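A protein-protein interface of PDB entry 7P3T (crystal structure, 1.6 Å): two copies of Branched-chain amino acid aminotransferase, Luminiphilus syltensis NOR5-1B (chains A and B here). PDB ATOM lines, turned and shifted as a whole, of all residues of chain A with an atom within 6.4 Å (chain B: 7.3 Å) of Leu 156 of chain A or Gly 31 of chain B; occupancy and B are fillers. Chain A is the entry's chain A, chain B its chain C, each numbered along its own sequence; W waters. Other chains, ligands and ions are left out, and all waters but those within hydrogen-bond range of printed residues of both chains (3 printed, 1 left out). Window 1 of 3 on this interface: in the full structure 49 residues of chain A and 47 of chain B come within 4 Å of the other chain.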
ATOM      1  N   GLN A  26     -15.160   2.044  16.097  1.00  0.00           N
ATOM      2  CA  GLN A  26     -15.901   2.918  15.177  1.00  0.00           C
ATOM      3  C   GLN A  26     -17.227   2.315  14.735  1.00  0.00           C
ATOM      4  O   GLN A  26     -18.116   3.051  14.268  1.00  0.00           O
ATOM      5  CB  GLN A  26     -15.015   3.247  13.976  1.00  0.00           C
ATOM      6  CG  GLN A  26     -13.859   4.155  14.347  1.00  0.00           C
ATOM      7  CD  GLN A  26     -12.808   4.268  13.269  1.00  0.00           C
ATOM      8  OE1 GLN A  26     -12.691   5.312  12.622  1.00  0.00           O
ATOM      9  NE2 GLN A  26     -12.004   3.212  13.094  1.00  0.00           N
ATOM     10  N   GLY A  27     -17.389   1.001  14.862  1.00  0.00           N
ATOM     11  CA  GLY A  27     -18.695   0.405  14.669  1.00  0.00           C
ATOM     12  C   GLY A  27     -19.701   0.879  15.699  1.00  0.00           C
ATOM     13  O   GLY A  27     -20.889   0.975  15.413  1.00  0.00           O
ATOM     14  N   PHE A  28     -19.236   1.151  16.917  1.00  0.00           N
ATOM     15  CA  PHE A  28     -20.085   1.627  18.002  1.00  0.00           C
ATOM     16  C   PHE A  28     -20.279   3.133  17.920  1.00  0.00           C
ATOM     17  O   PHE A  28     -21.411   3.617  17.899  1.00  0.00           O
ATOM     18  CB  PHE A  28     -19.453   1.233  19.348  1.00  0.00           C
ATOM     19  CG  PHE A  28     -20.235   1.672  20.557  1.00  0.00           C
ATOM     20  CD1 PHE A  28     -21.471   1.122  20.826  1.00  0.00           C
ATOM     21  CD2 PHE A  28     -19.733   2.603  21.430  1.00  0.00           C
ATOM     22  CE1 PHE A  28     -22.184   1.494  21.898  1.00  0.00           C
ATOM     23  CE2 PHE A  28     -20.468   2.995  22.539  1.00  0.00           C
ATOM     24  CZ  PHE A  28     -21.695   2.431  22.777  1.00  0.00           C
ATOM     25  N   GLY A  31     -21.238   3.884  13.838  1.00  0.00           N
ATOM     26  CA  GLY A  31     -22.012   3.006  12.976  1.00  0.00           C
ATOM     27  C   GLY A  31     -21.245   2.539  11.757  1.00  0.00           C
ATOM     28  O   GLY A  31     -21.855   2.191  10.745  1.00  0.00           O
ATOM     29  N   ASP A  32     -19.913   2.499  11.843  1.00  0.00           N
ATOM     30  CA  ASP A  32     -19.053   2.205  10.697  1.00  0.00           C
ATOM     31  C   ASP A  32     -18.850   0.696  10.622  1.00  0.00           C
ATOM     32  O   ASP A  32     -17.815   0.134  11.000  1.00  0.00           O
ATOM     33  CB  ASP A  32     -17.748   2.980  10.805  1.00  0.00           C
ATOM     34  CG  ASP A  32     -16.963   2.983   9.518  1.00  0.00           C
ATOM     35  OD1 ASP A  32     -17.367   2.262   8.577  1.00  0.00           O
ATOM     36  OD2 ASP A  32     -15.942   3.697   9.455  1.00  0.00           O
ATOM     37  N   GLY A  33     -19.875   0.032  10.112  1.00  0.00           N
ATOM     38  CA  GLY A  33     -19.835  -1.400   9.928  1.00  0.00           C
ATOM     39  C   GLY A  33     -21.017  -1.885   9.123  1.00  0.00           C
ATOM     40  O   GLY A  33     -22.035  -1.191   8.978  1.00  0.00           O
ATOM     41  N   VAL A  34     -20.865  -3.099   8.587  1.00  0.00           N
ATOM     42  CA  VAL A  34     -21.913  -3.757   7.823  1.00  0.00           C
ATOM     43  C   VAL A  34     -22.120  -5.151   8.392  1.00  0.00           C
ATOM     44  O   VAL A  34     -21.268  -5.696   9.101  1.00  0.00           O
ATOM     45  CB  VAL A  34     -21.589  -3.816   6.313  1.00  0.00           C
ATOM     46  CG1 VAL A  34     -21.445  -2.395   5.751  1.00  0.00           C
ATOM     47  CG2 VAL A  34     -20.326  -4.645   6.057  1.00  0.00           C
ATOM     48  N   PHE A  35     -23.273  -5.735   8.079  1.00  0.00           N
ATOM     49  CA  PHE A  35     -23.568  -7.060   8.602  1.00  0.00           C
ATOM     50  C   PHE A  35     -24.455  -7.828   7.639  1.00  0.00           C
ATOM     51  O   PHE A  35     -25.018  -7.276   6.692  1.00  0.00           O
ATOM     52  CB  PHE A  35     -24.227  -6.974   9.983  1.00  0.00           C
ATOM     53  CG  PHE A  35     -25.702  -6.612   9.969  1.00  0.00           C
ATOM     54  CD1 PHE A  35     -26.125  -5.297   9.877  1.00  0.00           C
ATOM     55  CD2 PHE A  35     -26.675  -7.595  10.066  1.00  0.00           C
ATOM     56  CE1 PHE A  35     -27.447  -4.984   9.888  1.00  0.00           C
ATOM     57  CE2 PHE A  35     -28.013  -7.275  10.070  1.00  0.00           C
ATOM     58  CZ  PHE A  35     -28.405  -5.963   9.977  1.00  0.00           C
ATOM     59  N   ILE A  94     -20.741  -9.710  11.333  1.00  0.00           N
ATOM     60  CA  ILE A  94     -20.545  -8.270  11.404  1.00  0.00           C
ATOM     61  C   ILE A  94     -19.077  -7.955  11.164  1.00  0.00           C
ATOM     62  O   ILE A  94     -18.196  -8.575  11.766  1.00  0.00           O
ATOM     63  CB  ILE A  94     -20.970  -7.706  12.779  1.00  0.00           C
ATOM     64  CG1 ILE A  94     -22.425  -8.034  13.083  1.00  0.00           C
ATOM     65  CG2 ILE A  94     -20.682  -6.216  12.835  1.00  0.00           C
ATOM     66  CD1 ILE A  94     -22.639  -8.350  14.528  1.00  0.00           C
ATOM     67  N   VAL A  95     -18.808  -6.948  10.339  1.00  0.00           N
ATOM     68  CA  VAL A  95     -17.482  -6.371  10.306  1.00  0.00           C
ATOM     69  C   VAL A  95     -17.594  -4.870  10.511  1.00  0.00           C
ATOM     70  O   VAL A  95     -18.450  -4.215   9.903  1.00  0.00           O
ATOM     71  CB  VAL A  95     -16.728  -6.727   9.000  1.00  0.00           C
ATOM     72  CG1 VAL A  95     -17.412  -6.182   7.742  1.00  0.00           C
ATOM     73  CG2 VAL A  95     -15.286  -6.293   9.096  1.00  0.00           C
ATOM     74  N   THR A  96     -16.710  -4.326  11.342  1.00  0.00           N
ATOM     75  CA  THR A  96     -16.636  -2.883  11.545  1.00  0.00           C
ATOM     76  C   THR A  96     -15.240  -2.370  11.229  1.00  0.00           C
ATOM     77  O   THR A  96     -14.262  -3.138  11.162  1.00  0.00           O
ATOM     78  CB  THR A  96     -16.994  -2.462  12.972  1.00  0.00           C
ATOM     79  OG1 THR A  96     -15.836  -2.546  13.821  1.00  0.00           O
ATOM     80  CG2 THR A  96     -18.120  -3.283  13.552  1.00  0.00           C
ATOM     81  N   LYS A 154     -26.719  -3.319   4.104  1.00  0.00           N
ATOM     82  CA  LYS A 154     -27.173  -3.937   5.336  1.00  0.00           C
ATOM     83  C   LYS A 154     -26.122  -3.528   6.359  1.00  0.00           C
ATOM     84  O   LYS A 154     -25.001  -4.048   6.344  1.00  0.00           O
ATOM     85  CB  LYS A 154     -27.295  -5.448   5.211  1.00  0.00           C
ATOM     86  CG  LYS A 154     -28.342  -6.030   6.147  1.00  0.00           C
ATOM     87  CD  LYS A 154     -28.694  -7.481   5.801  1.00  0.00           C
ATOM     88  CE  LYS A 154     -29.751  -8.017   6.742  1.00  0.00           C
ATOM     89  NZ  LYS A 154     -31.093  -7.380   6.536  1.00  0.00           N
ATOM     90  N   CYS A 155     -26.448  -2.540   7.192  1.00  0.00           N
ATOM     91  CA  CYS A 155     -25.421  -1.915   8.022  1.00  0.00           C
ATOM     92  C   CYS A 155     -25.972  -1.580   9.396  1.00  0.00           C
ATOM     93  O   CYS A 155     -27.159  -1.756   9.691  1.00  0.00           O
ATOM     94  CB  CYS A 155     -24.856  -0.662   7.347  1.00  0.00           C
ATOM     95  SG  CYS A 155     -25.986   0.738   7.246  1.00  0.00           S
ATOM     96  N   LEU A 156     -25.068  -1.131  10.263  1.00  0.00           N
ATOM     97  CA  LEU A 156     -25.387  -0.940  11.660  1.00  0.00           C
ATOM     98  C   LEU A 156     -26.225   0.303  11.928  1.00  0.00           C
ATOM     99  O   LEU A 156     -26.645   0.518  13.064  1.00  0.00           O
ATOM    100  CB  LEU A 156     -24.098  -0.877  12.477  1.00  0.00           C
ATOM    101  CG  LEU A 156     -23.105  -2.028  12.290  1.00  0.00           C
ATOM    102  CD1 LEU A 156     -21.876  -1.753  13.116  1.00  0.00           C
ATOM    103  CD2 LEU A 156     -23.724  -3.350  12.698  1.00  0.00           C
ATOM    104  N   ASP A 157     -26.558   1.078  10.907  1.00  0.00           N
ATOM    105  CA  ASP A 157     -27.094   2.420  11.092  1.00  0.00           C
ATOM    106  C   ASP A 157     -28.610   2.358  11.003  1.00  0.00           C
ATOM    107  O   ASP A 157     -29.213   2.680   9.980  1.00  0.00           O
ATOM    108  CB  ASP A 157     -26.503   3.365  10.057  1.00  0.00           C
ATOM    109  CG  ASP A 157     -24.984   3.459  10.160  1.00  0.00           C
ATOM    110  OD1 ASP A 157     -24.340   2.377  10.183  1.00  0.00           O
ATOM    111  OD2 ASP A 157     -24.443   4.587  10.244  1.00  0.00           O
ATOM    112  N   ARG A 158     -29.231   1.945  12.114  1.00  0.00           N
ATOM    113  CA  ARG A 158     -30.649   1.605  12.099  1.00  0.00           C
ATOM    114  C   ARG A 158     -31.452   2.325  13.182  1.00  0.00           C
ATOM    115  O   ARG A 158     -32.570   1.912  13.495  1.00  0.00           O
ATOM    116  CB  ARG A 158     -30.811   0.080  12.184  1.00  0.00           C
ATOM    117  CG  ARG A 158     -30.343  -0.627  10.934  1.00  0.00           C
ATOM    118  CD  ARG A 158     -30.091  -2.120  11.049  1.00  0.00           C
ATOM    119  NE  ARG A 158     -31.302  -2.924  10.979  1.00  0.00           N
ATOM    120  CZ  ARG A 158     -31.785  -3.483   9.858  1.00  0.00           C
ATOM    121  NH1 ARG A 158     -32.893  -4.196   9.921  1.00  0.00           N
ATOM    122  NH2 ARG A 158     -31.156  -3.341   8.700  1.00  0.00           N
ATOM    123  N   LEU A 159     -30.960   3.453  13.708  1.00  0.00           N
ATOM    124  CA  LEU A 159     -31.780   4.240  14.612  1.00  0.00           C
ATOM    125  C   LEU A 159     -33.099   4.626  13.939  1.00  0.00           C
ATOM    126  O   LEU A 159     -34.159   4.581  14.569  1.00  0.00           O
ATOM    127  CB  LEU A 159     -31.011   5.482  15.071  1.00  0.00           C
ATOM    128  CG  LEU A 159     -31.789   6.460  15.940  1.00  0.00           C
ATOM    129  CD1 LEU A 159     -32.329   5.808  17.209  1.00  0.00           C
ATOM    130  CD2 LEU A 159     -30.916   7.654  16.316  1.00  0.00           C
ATOM    131  N   HIS A 160     -33.028   4.983  12.650  1.00  0.00           N
ATOM    132  CA  HIS A 160     -34.175   5.240  11.769  1.00  0.00           C
ATOM    133  C   HIS A 160     -35.277   4.213  11.984  1.00  0.00           C
ATOM    134  O   HIS A 160     -36.422   4.568  12.275  1.00  0.00           O
ATOM    135  CB  HIS A 160     -33.618   5.267  10.318  1.00  0.00           C
ATOM    136  CG  HIS A 160     -34.602   5.041   9.195  1.00  0.00           C
ATOM    137  ND1 HIS A 160     -34.780   3.807   8.604  1.00  0.00           N
ATOM    138  CD2 HIS A 160     -35.354   5.911   8.473  1.00  0.00           C
ATOM    139  CE1 HIS A 160     -35.660   3.910   7.620  1.00  0.00           C
ATOM    140  NE2 HIS A 160     -36.011   5.180   7.509  1.00  0.00           N
ATOM    141  N   GLN A 162     -35.457   1.824  14.353  1.00  0.00           N
ATOM    142  CA  GLN A 162     -35.822   1.703  15.754  1.00  0.00           C
ATOM    143  C   GLN A 162     -36.920   2.688  16.133  1.00  0.00           C
ATOM    144  O   GLN A 162     -37.847   2.338  16.868  1.00  0.00           O
ATOM    145  CB  GLN A 162     -34.599   1.921  16.637  1.00  0.00           C
ATOM    146  CG  GLN A 162     -33.620   0.799  16.548  1.00  0.00           C
ATOM    147  CD  GLN A 162     -34.164  -0.462  17.153  1.00  0.00           C
ATOM    148  OE1 GLN A 162     -34.751  -1.282  16.455  1.00  0.00           O
ATOM    149  NE2 GLN A 162     -33.984  -0.627  18.463  1.00  0.00           N
ATOM    150  N   ASP B  25     -25.215  -5.035  22.291  1.00  0.00           N
ATOM    151  CA  ASP B  25     -25.727  -3.710  22.617  1.00  0.00           C
ATOM    152  C   ASP B  25     -26.394  -3.124  21.381  1.00  0.00           C
ATOM    153  O   ASP B  25     -25.855  -3.220  20.279  1.00  0.00           O
ATOM    154  CB  ASP B  25     -24.594  -2.817  23.082  1.00  0.00           C
ATOM    155  CG  ASP B  25     -25.088  -1.576  23.795  1.00  0.00           C
ATOM    156  OD1 ASP B  25     -25.590  -0.637  23.123  1.00  0.00           O
ATOM    157  OD2 ASP B  25     -24.963  -1.546  25.030  1.00  0.00           O
ATOM    158  N   GLN B  26     -27.614  -2.596  21.540  1.00  0.00           N
ATOM    159  CA  GLN B  26     -28.332  -2.061  20.399  1.00  0.00           C
ATOM    160  C   GLN B  26     -27.690  -0.792  19.866  1.00  0.00           C
ATOM    161  O   GLN B  26     -27.940  -0.417  18.716  1.00  0.00           O
ATOM    162  CB  GLN B  26     -29.790  -1.800  20.794  1.00  0.00           C
ATOM    163  CG  GLN B  26     -30.577  -3.082  20.984  1.00  0.00           C
ATOM    164  CD  GLN B  26     -31.953  -2.874  21.609  1.00  0.00           C
ATOM    165  OE1 GLN B  26     -32.970  -2.949  20.922  1.00  0.00           O
ATOM    166  NE2 GLN B  26     -31.991  -2.668  22.928  1.00  0.00           N
ATOM    167  N   GLY B  27     -26.848  -0.138  20.665  1.00  0.00           N
ATOM    168  CA  GLY B  27     -26.070   0.958  20.130  1.00  0.00           C
ATOM    169  C   GLY B  27     -25.025   0.478  19.145  1.00  0.00           C
ATOM    170  O   GLY B  27     -24.670   1.201  18.207  1.00  0.00           O
ATOM    171  N   PHE B  28     -24.548  -0.754  19.323  1.00  0.00           N
ATOM    172  CA  PHE B  28     -23.584  -1.345  18.396  1.00  0.00           C
ATOM    173  C   PHE B  28     -24.275  -1.959  17.190  1.00  0.00           C
ATOM    174  O   PHE B  28     -23.902  -1.685  16.045  1.00  0.00           O
ATOM    175  CB  PHE B  28     -22.754  -2.414  19.115  1.00  0.00           C
ATOM    176  CG  PHE B  28     -21.710  -3.078  18.255  1.00  0.00           C
ATOM    177  CD1 PHE B  28     -20.605  -2.364  17.790  1.00  0.00           C
ATOM    178  CD2 PHE B  28     -21.805  -4.424  17.934  1.00  0.00           C
ATOM    179  CE1 PHE B  28     -19.628  -3.009  17.006  1.00  0.00           C
ATOM    180  CE2 PHE B  28     -20.853  -5.050  17.153  1.00  0.00           C
ATOM    181  CZ  PHE B  28     -19.745  -4.349  16.703  1.00  0.00           C
ATOM    182  N   LEU B  29     -25.259  -2.832  17.426  1.00  0.00           N
ATOM    183  CA  LEU B  29     -25.863  -3.573  16.326  1.00  0.00           C
ATOM    184  C   LEU B  29     -26.752  -2.709  15.458  1.00  0.00           C
ATOM    185  O   LEU B  29     -26.940  -3.023  14.281  1.00  0.00           O
ATOM    186  CB  LEU B  29     -26.698  -4.730  16.844  1.00  0.00           C
ATOM    187  CG  LEU B  29     -25.958  -5.843  17.559  1.00  0.00           C
ATOM    188  CD1 LEU B  29     -26.998  -6.860  18.063  1.00  0.00           C
ATOM    189  CD2 LEU B  29     -24.977  -6.547  16.653  1.00  0.00           C
ATOM    190  N   LEU B  30     -27.394  -1.703  16.043  1.00  0.00           N
ATOM    191  CA  LEU B  30     -28.424  -0.948  15.347  1.00  0.00           C
ATOM    192  C   LEU B  30     -28.198   0.550  15.375  1.00  0.00           C
ATOM    193  O   LEU B  30     -29.065   1.296  14.904  1.00  0.00           O
ATOM    194  CB  LEU B  30     -29.795  -1.223  15.952  1.00  0.00           C
ATOM    195  CG  LEU B  30     -30.223  -2.675  16.058  1.00  0.00           C
ATOM    196  CD1 LEU B  30     -31.575  -2.767  16.785  1.00  0.00           C
ATOM    197  CD2 LEU B  30     -30.298  -3.314  14.703  1.00  0.00           C
ATOM    198  N   GLY B  31     -27.087   1.019  15.924  1.00  0.00           N
ATOM    199  CA  GLY B  31     -26.871   2.460  16.018  1.00  0.00           C
ATOM    200  C   GLY B  31     -27.907   3.173  16.860  1.00  0.00           C
ATOM    201  O   GLY B  31     -28.183   4.355  16.649  1.00  0.00           O
ATOM    202  N   ASP B  32     -28.476   2.482  17.831  1.00  0.00           N
ATOM    203  CA  ASP B  32     -29.580   3.020  18.625  1.00  0.00           C
ATOM    204  C   ASP B  32     -29.010   3.747  19.833  1.00  0.00           C
ATOM    205  O   ASP B  32     -28.972   3.240  20.959  1.00  0.00           O
ATOM    206  CB  ASP B  32     -30.516   1.889  19.012  1.00  0.00           C
ATOM    207  CG  ASP B  32     -31.824   2.375  19.529  1.00  0.00           C
ATOM    208  OD1 ASP B  32     -31.969   3.608  19.736  1.00  0.00           O
ATOM    209  OD2 ASP B  32     -32.698   1.509  19.763  1.00  0.00           O
ATOM    210  N   GLY B  33     -28.551   4.960  19.574  1.00  0.00           N
ATOM    211  CA  GLY B  33     -27.907   5.749  20.605  1.00  0.00           C
ATOM    212  C   GLY B  33     -27.644   7.145  20.103  1.00  0.00           C
ATOM    213  O   GLY B  33     -27.614   7.408  18.894  1.00  0.00           O
ATOM    214  N   VAL B  34     -27.474   8.050  21.062  1.00  0.00           N
ATOM    215  CA  VAL B  34     -27.181   9.445  20.781  1.00  0.00           C
ATOM    216  C   VAL B  34     -25.987   9.855  21.629  1.00  0.00           C
ATOM    217  O   VAL B  34     -25.624   9.194  22.599  1.00  0.00           O
ATOM    218  CB  VAL B  34     -28.381  10.386  21.040  1.00  0.00           C
ATOM    219  CG1 VAL B  34     -29.563  10.022  20.132  1.00  0.00           C
ATOM    220  CG2 VAL B  34     -28.823  10.366  22.474  1.00  0.00           C
ATOM    221  N   LEU B  64     -35.120   7.883  24.336  1.00  0.00           N
ATOM    222  CA  LEU B  64     -34.086   7.242  25.141  1.00  0.00           C
ATOM    223  C   LEU B  64     -34.112   7.708  26.597  1.00  0.00           C
ATOM    224  O   LEU B  64     -33.110   7.570  27.310  1.00  0.00           O
ATOM    225  CB  LEU B  64     -32.727   7.482  24.501  1.00  0.00           C
ATOM    226  CG  LEU B  64     -32.404   6.593  23.292  1.00  0.00           C
ATOM    227  CD1 LEU B  64     -31.220   7.140  22.485  1.00  0.00           C
ATOM    228  CD2 LEU B  64     -32.147   5.149  23.710  1.00  0.00           C
ATOM    229  N   THR B  96     -27.092   4.669  24.918  1.00  0.00           N
ATOM    230  CA  THR B  96     -27.697   3.756  23.966  1.00  0.00           C
ATOM    231  C   THR B  96     -28.869   3.026  24.599  1.00  0.00           C
ATOM    232  O   THR B  96     -29.020   2.952  25.816  1.00  0.00           O
ATOM    233  CB  THR B  96     -26.706   2.698  23.434  1.00  0.00           C
ATOM    234  OG1 THR B  96     -26.641   1.590  24.337  1.00  0.00           O
ATOM    235  CG2 THR B  96     -25.314   3.298  23.227  1.00  0.00           C
ATOM    236  N   ARG B  97     -29.666   2.402  23.737  1.00  0.00           N
ATOM    237  CA  ARG B  97     -30.796   1.582  24.171  1.00  0.00           C
ATOM    238  C   ARG B  97     -30.344   0.289  24.848  1.00  0.00           C
ATOM    239  O   ARG B  97     -31.185  -0.444  25.364  1.00  0.00           O
ATOM    240  CB  ARG B  97     -31.716   1.313  22.974  1.00  0.00           C
ATOM    241  CG  ARG B  97     -33.061   0.702  23.378  1.00  0.00           C
ATOM    242  CD  ARG B  97     -34.326   1.372  22.837  1.00  0.00           C
ATOM    243  NE  ARG B  97     -34.130   2.252  21.687  1.00  0.00           N
ATOM    244  CZ  ARG B  97     -34.593   3.499  21.605  1.00  0.00           C
ATOM    245  NH1 ARG B  97     -35.321   3.983  22.598  1.00  0.00           N
ATOM    246  NH2 ARG B  97     -34.369   4.244  20.530  1.00  0.00           N
ATOM    247  N   LEU B 149     -33.601  10.397   8.834  1.00  0.00           N
ATOM    248  CA  LEU B 149     -32.898  10.462  10.103  1.00  0.00           C
ATOM    249  C   LEU B 149     -32.520  11.933  10.239  1.00  0.00           C
ATOM    250  O   LEU B 149     -31.554  12.373   9.620  1.00  0.00           O
ATOM    251  CB  LEU B 149     -31.682   9.553  10.131  1.00  0.00           C
ATOM    252  CG  LEU B 149     -30.975   9.585  11.479  1.00  0.00           C
ATOM    253  CD1 LEU B 149     -31.844   9.007  12.604  1.00  0.00           C
ATOM    254  CD2 LEU B 149     -29.627   8.845  11.354  1.00  0.00           C
ATOM    255  N   CYS B 155     -25.979  11.517  16.648  1.00  0.00           N
ATOM    256  CA  CYS B 155     -26.208  10.110  16.956  1.00  0.00           C
ATOM    257  C   CYS B 155     -25.104   9.240  16.374  1.00  0.00           C
ATOM    258  O   CYS B 155     -24.219   9.699  15.651  1.00  0.00           O
ATOM    259  CB  CYS B 155     -27.583   9.649  16.459  1.00  0.00           C
ATOM    260  SG  CYS B 155     -27.794   9.572  14.720  1.00  0.00           S
ATOM    261  N   LEU B 156     -25.180   7.952  16.696  1.00  0.00           N
ATOM    262  CA  LEU B 156     -24.116   7.008  16.363  1.00  0.00           C
ATOM    263  C   LEU B 156     -24.110   6.595  14.896  1.00  0.00           C
ATOM    264  O   LEU B 156     -23.230   5.838  14.478  1.00  0.00           O
ATOM    265  CB  LEU B 156     -24.248   5.761  17.239  1.00  0.00           C
ATOM    266  CG  LEU B 156     -24.257   5.941  18.753  1.00  0.00           C
ATOM    267  CD1 LEU B 156     -24.338   4.608  19.493  1.00  0.00           C
ATOM    268  CD2 LEU B 156     -22.991   6.715  19.158  1.00  0.00           C
ATOM    269  N   ASP B 157     -25.050   7.082  14.092  1.00  0.00           N
ATOM    270  CA  ASP B 157     -25.294   6.555  12.757  1.00  0.00           C
ATOM    271  C   ASP B 157     -24.576   7.411  11.720  1.00  0.00           C
ATOM    272  O   ASP B 157     -25.164   8.278  11.062  1.00  0.00           O
ATOM    273  CB  ASP B 157     -26.800   6.520  12.510  1.00  0.00           C
ATOM    274  CG  ASP B 157     -27.527   5.652  13.513  1.00  0.00           C
ATOM    275  OD1 ASP B 157     -27.376   5.853  14.743  1.00  0.00           O
ATOM    276  OD2 ASP B 157     -28.263   4.755  13.068  1.00  0.00           O
ATOM    277  N   LEU B 159     -22.012   6.107   9.315  1.00  0.00           N
ATOM    278  CA  LEU B 159     -21.362   5.478   8.176  1.00  0.00           C
ATOM    279  C   LEU B 159     -21.382   6.412   6.960  1.00  0.00           C
ATOM    280  O   LEU B 159     -20.378   6.529   6.246  1.00  0.00           O
ATOM    281  CB  LEU B 159     -22.040   4.146   7.854  1.00  0.00           C
ATOM    282  CG  LEU B 159     -21.553   3.449   6.593  1.00  0.00           C
ATOM    283  CD1 LEU B 159     -20.057   3.162   6.656  1.00  0.00           C
ATOM    284  CD2 LEU B 159     -22.330   2.148   6.344  1.00  0.00           C
HETATM  285  O   HOH W   1     -30.456   5.137  11.022  1.00  0.00           O
HETATM  286  O   HOH W   2     -24.990   3.295  13.609  1.00  0.00           O
HETATM  287  O   HOH W   3     -25.059   6.901   8.448  1.00  0.00           O
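O of Gly 33 of chain A is in hydrogen-bond range of N of Leu 156 of chain A (3.3 Å). N of Asp 32 of chain B sits at hydrogen-bond distance from O of Gln 26 of chain B, 3.1 Å away. The backbone carbonyl oxygen of Gly 31 of chain A sits close to the side-chain carboxylate of Asp 157 of chain A (2.6 Å). The side-chain sulfur (SG) of Cys 155 of chain A lies close to the backbone NH (N) of Asp 157 of chain A (3.7 Å). The backbone NH of Gly 27 of chain B lies within hydrogen-bond range of the side-chain carboxylate of Asp 25 of chain B (2.8 Å).
Water W1 lies within hydrogen-bond range of the backbone carbonyl oxygen of Asp 157 of chain A (2.9 Å), the side-chain carboxylate of Asp 157 of chain B (3.0 Å), the backbone NH of His 160 of chain A (3.0 Å) and the backbone NH of Leu 159 of chain A (3.2 Å). Water W3 lies within hydrogen-bond range of the backbone carbonyl oxygen of Asp 157 of chain B (3.0 Å), the side-chain carboxylate of Asp 157 of chain A (3.0 Å) and the backbone NH of Leu 159 of chain B (3.3 Å).
Among the printed residues, pairs that only touch across the chains: Gly 27 of chain A with Phe 28 of chain B, Phe 28 of chain A with Gly 27 of chain B, Phe 28 of chain A with Phe 28 of chain B, Phe 28 of chain A with Thr 96 of chain B, Phe 28 of chain A with Leu 156 of chain B, Gly 31 of chain A with Leu 159 of chain B, Asp 32 of chain A with Leu 159 of chain B, Ile 94 of chain A with Leu 29 of chain B, Thr 96 of chain A with Phe 28 of chain B, Cys 155 of chain A with Leu 159 of chain B, Leu 156 of chain A with Phe 28 of chain B, Leu 156 of chain A with Leu 29 of chain B, Asp 157 of chain A with Asp 157 of chain B, Leu 159 of chain A with Gly 31 of chain B, Leu 159 of chain A with Asp 32 of chain B, Leu 159 of chain A with Cys 155 of chain B, Gln 162 of chain A with Gln 26 of chain B and Gln 162 of chain A with Leu 30 of chain B.
Printed residues of chain A that touch a printed residue of chain B: Gly 27, Phe 28, Gly 31, Asp 32, Ile 94, Thr 96, Cys 155, Leu 156, Asp 157, Arg 158, Leu 159 and Gln 162. Among the printed residues, 27 pairs touch across the chains. Among the printed residues, no Asp or Glu carboxylate lies within 4 Å of a Lys or Arg side-chain nitrogen of the other chain.
Gln 26 of chain A touches none of the printed residues of chain B. Of chain B, only Phe 28, Leu 29, Leu 30 and Gly 31 come within 4 Å of Leu 156 of chain A. Of the printed residues of chain B, Arg 158 of chain A touches Leu 30 and Asp 157. Printed residues of chain B within 4 Å of Gln 162 of chain A: Gln 26 (3.5 Å), Leu 30 (3.5 Å) and Asp 32 (2.8 Å). Printed residues of chain A within 4 Å of Gly 27 of chain B: Phe 28 (3.98 Å). Of the printed residues of chain A, Leu 29 of chain B touches Ile 94 (3.6 Å) and Leu 156 (3.6 Å). Printed residues of chain A within 4 Å of Gly 31 of chain B: Leu 156 (2.9 Å) and Leu 159 (3.4 Å). The nearest residue of chain B that does not touch Leu 156 of chain A is Asp 157 of chain B (4.5 Å). The nearest residue of chain A that does not touch Gly 31 of chain B is Arg 158 of chain A (4.5 Å). The nearest printed residue of chain B that does not touch Gly 31 of chain A is Asp 157 of chain B (4.8 Å).
The backbone NH (N) of Arg 158 of chain A is in hydrogen-bond range of the side-chain carboxylate (OD2) of Asp 157 of chain B, 3.1 Å away. OD2 of Asp 157 of chain A is in hydrogen-bond range of N of Leu 159 of chain B (3.0 Å). N of Gly 31 of chain A is in hydrogen-bond range of O of Leu 156 of chain B (2.9 Å). N of Leu 159 of chain A lies within hydrogen-bond range of OD2 of Asp 157 of chain B, 3.1 Å away. The backbone carbonyl oxygen (O) of Leu 30 of chain B is in hydrogen-bond range of the backbone NH (N) of Leu 159 of chain A. The backbone carbonyl oxygen of Leu 156 of chain A sits close to the backbone carbonyl oxygen of Leu 30 of chain B, at 3.1 Å. N of Arg 158 of chain A sits at hydrogen-bond distance from O of Leu 30 of chain B. O of Leu 156 of chain A is in hydrogen-bond range of N of Gly 31 of chain B (2.9 Å). OD2 of Asp 32 of chain B is in hydrogen-bond range of NE2 of Gln 162 of chain A (2.8 Å).
Phe 28 of chain A touches Thr 96 of chain B, and with the chains exchanged Thr 96 of chain A touches Phe 28 of chain B. Phe 28 of chain A touches Leu 156 of chain B, and with the chains exchanged Leu 156 of chain A touches Phe 28 of chain B. Asp 32 of chain A touches Leu 159 of chain B, and with the chains exchanged Leu 159 of chain A touches Asp 32 of chain B. Of the 27 pairs that touch across the chains among the printed residues, 18 have their exchanged pair printed and touching as well.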
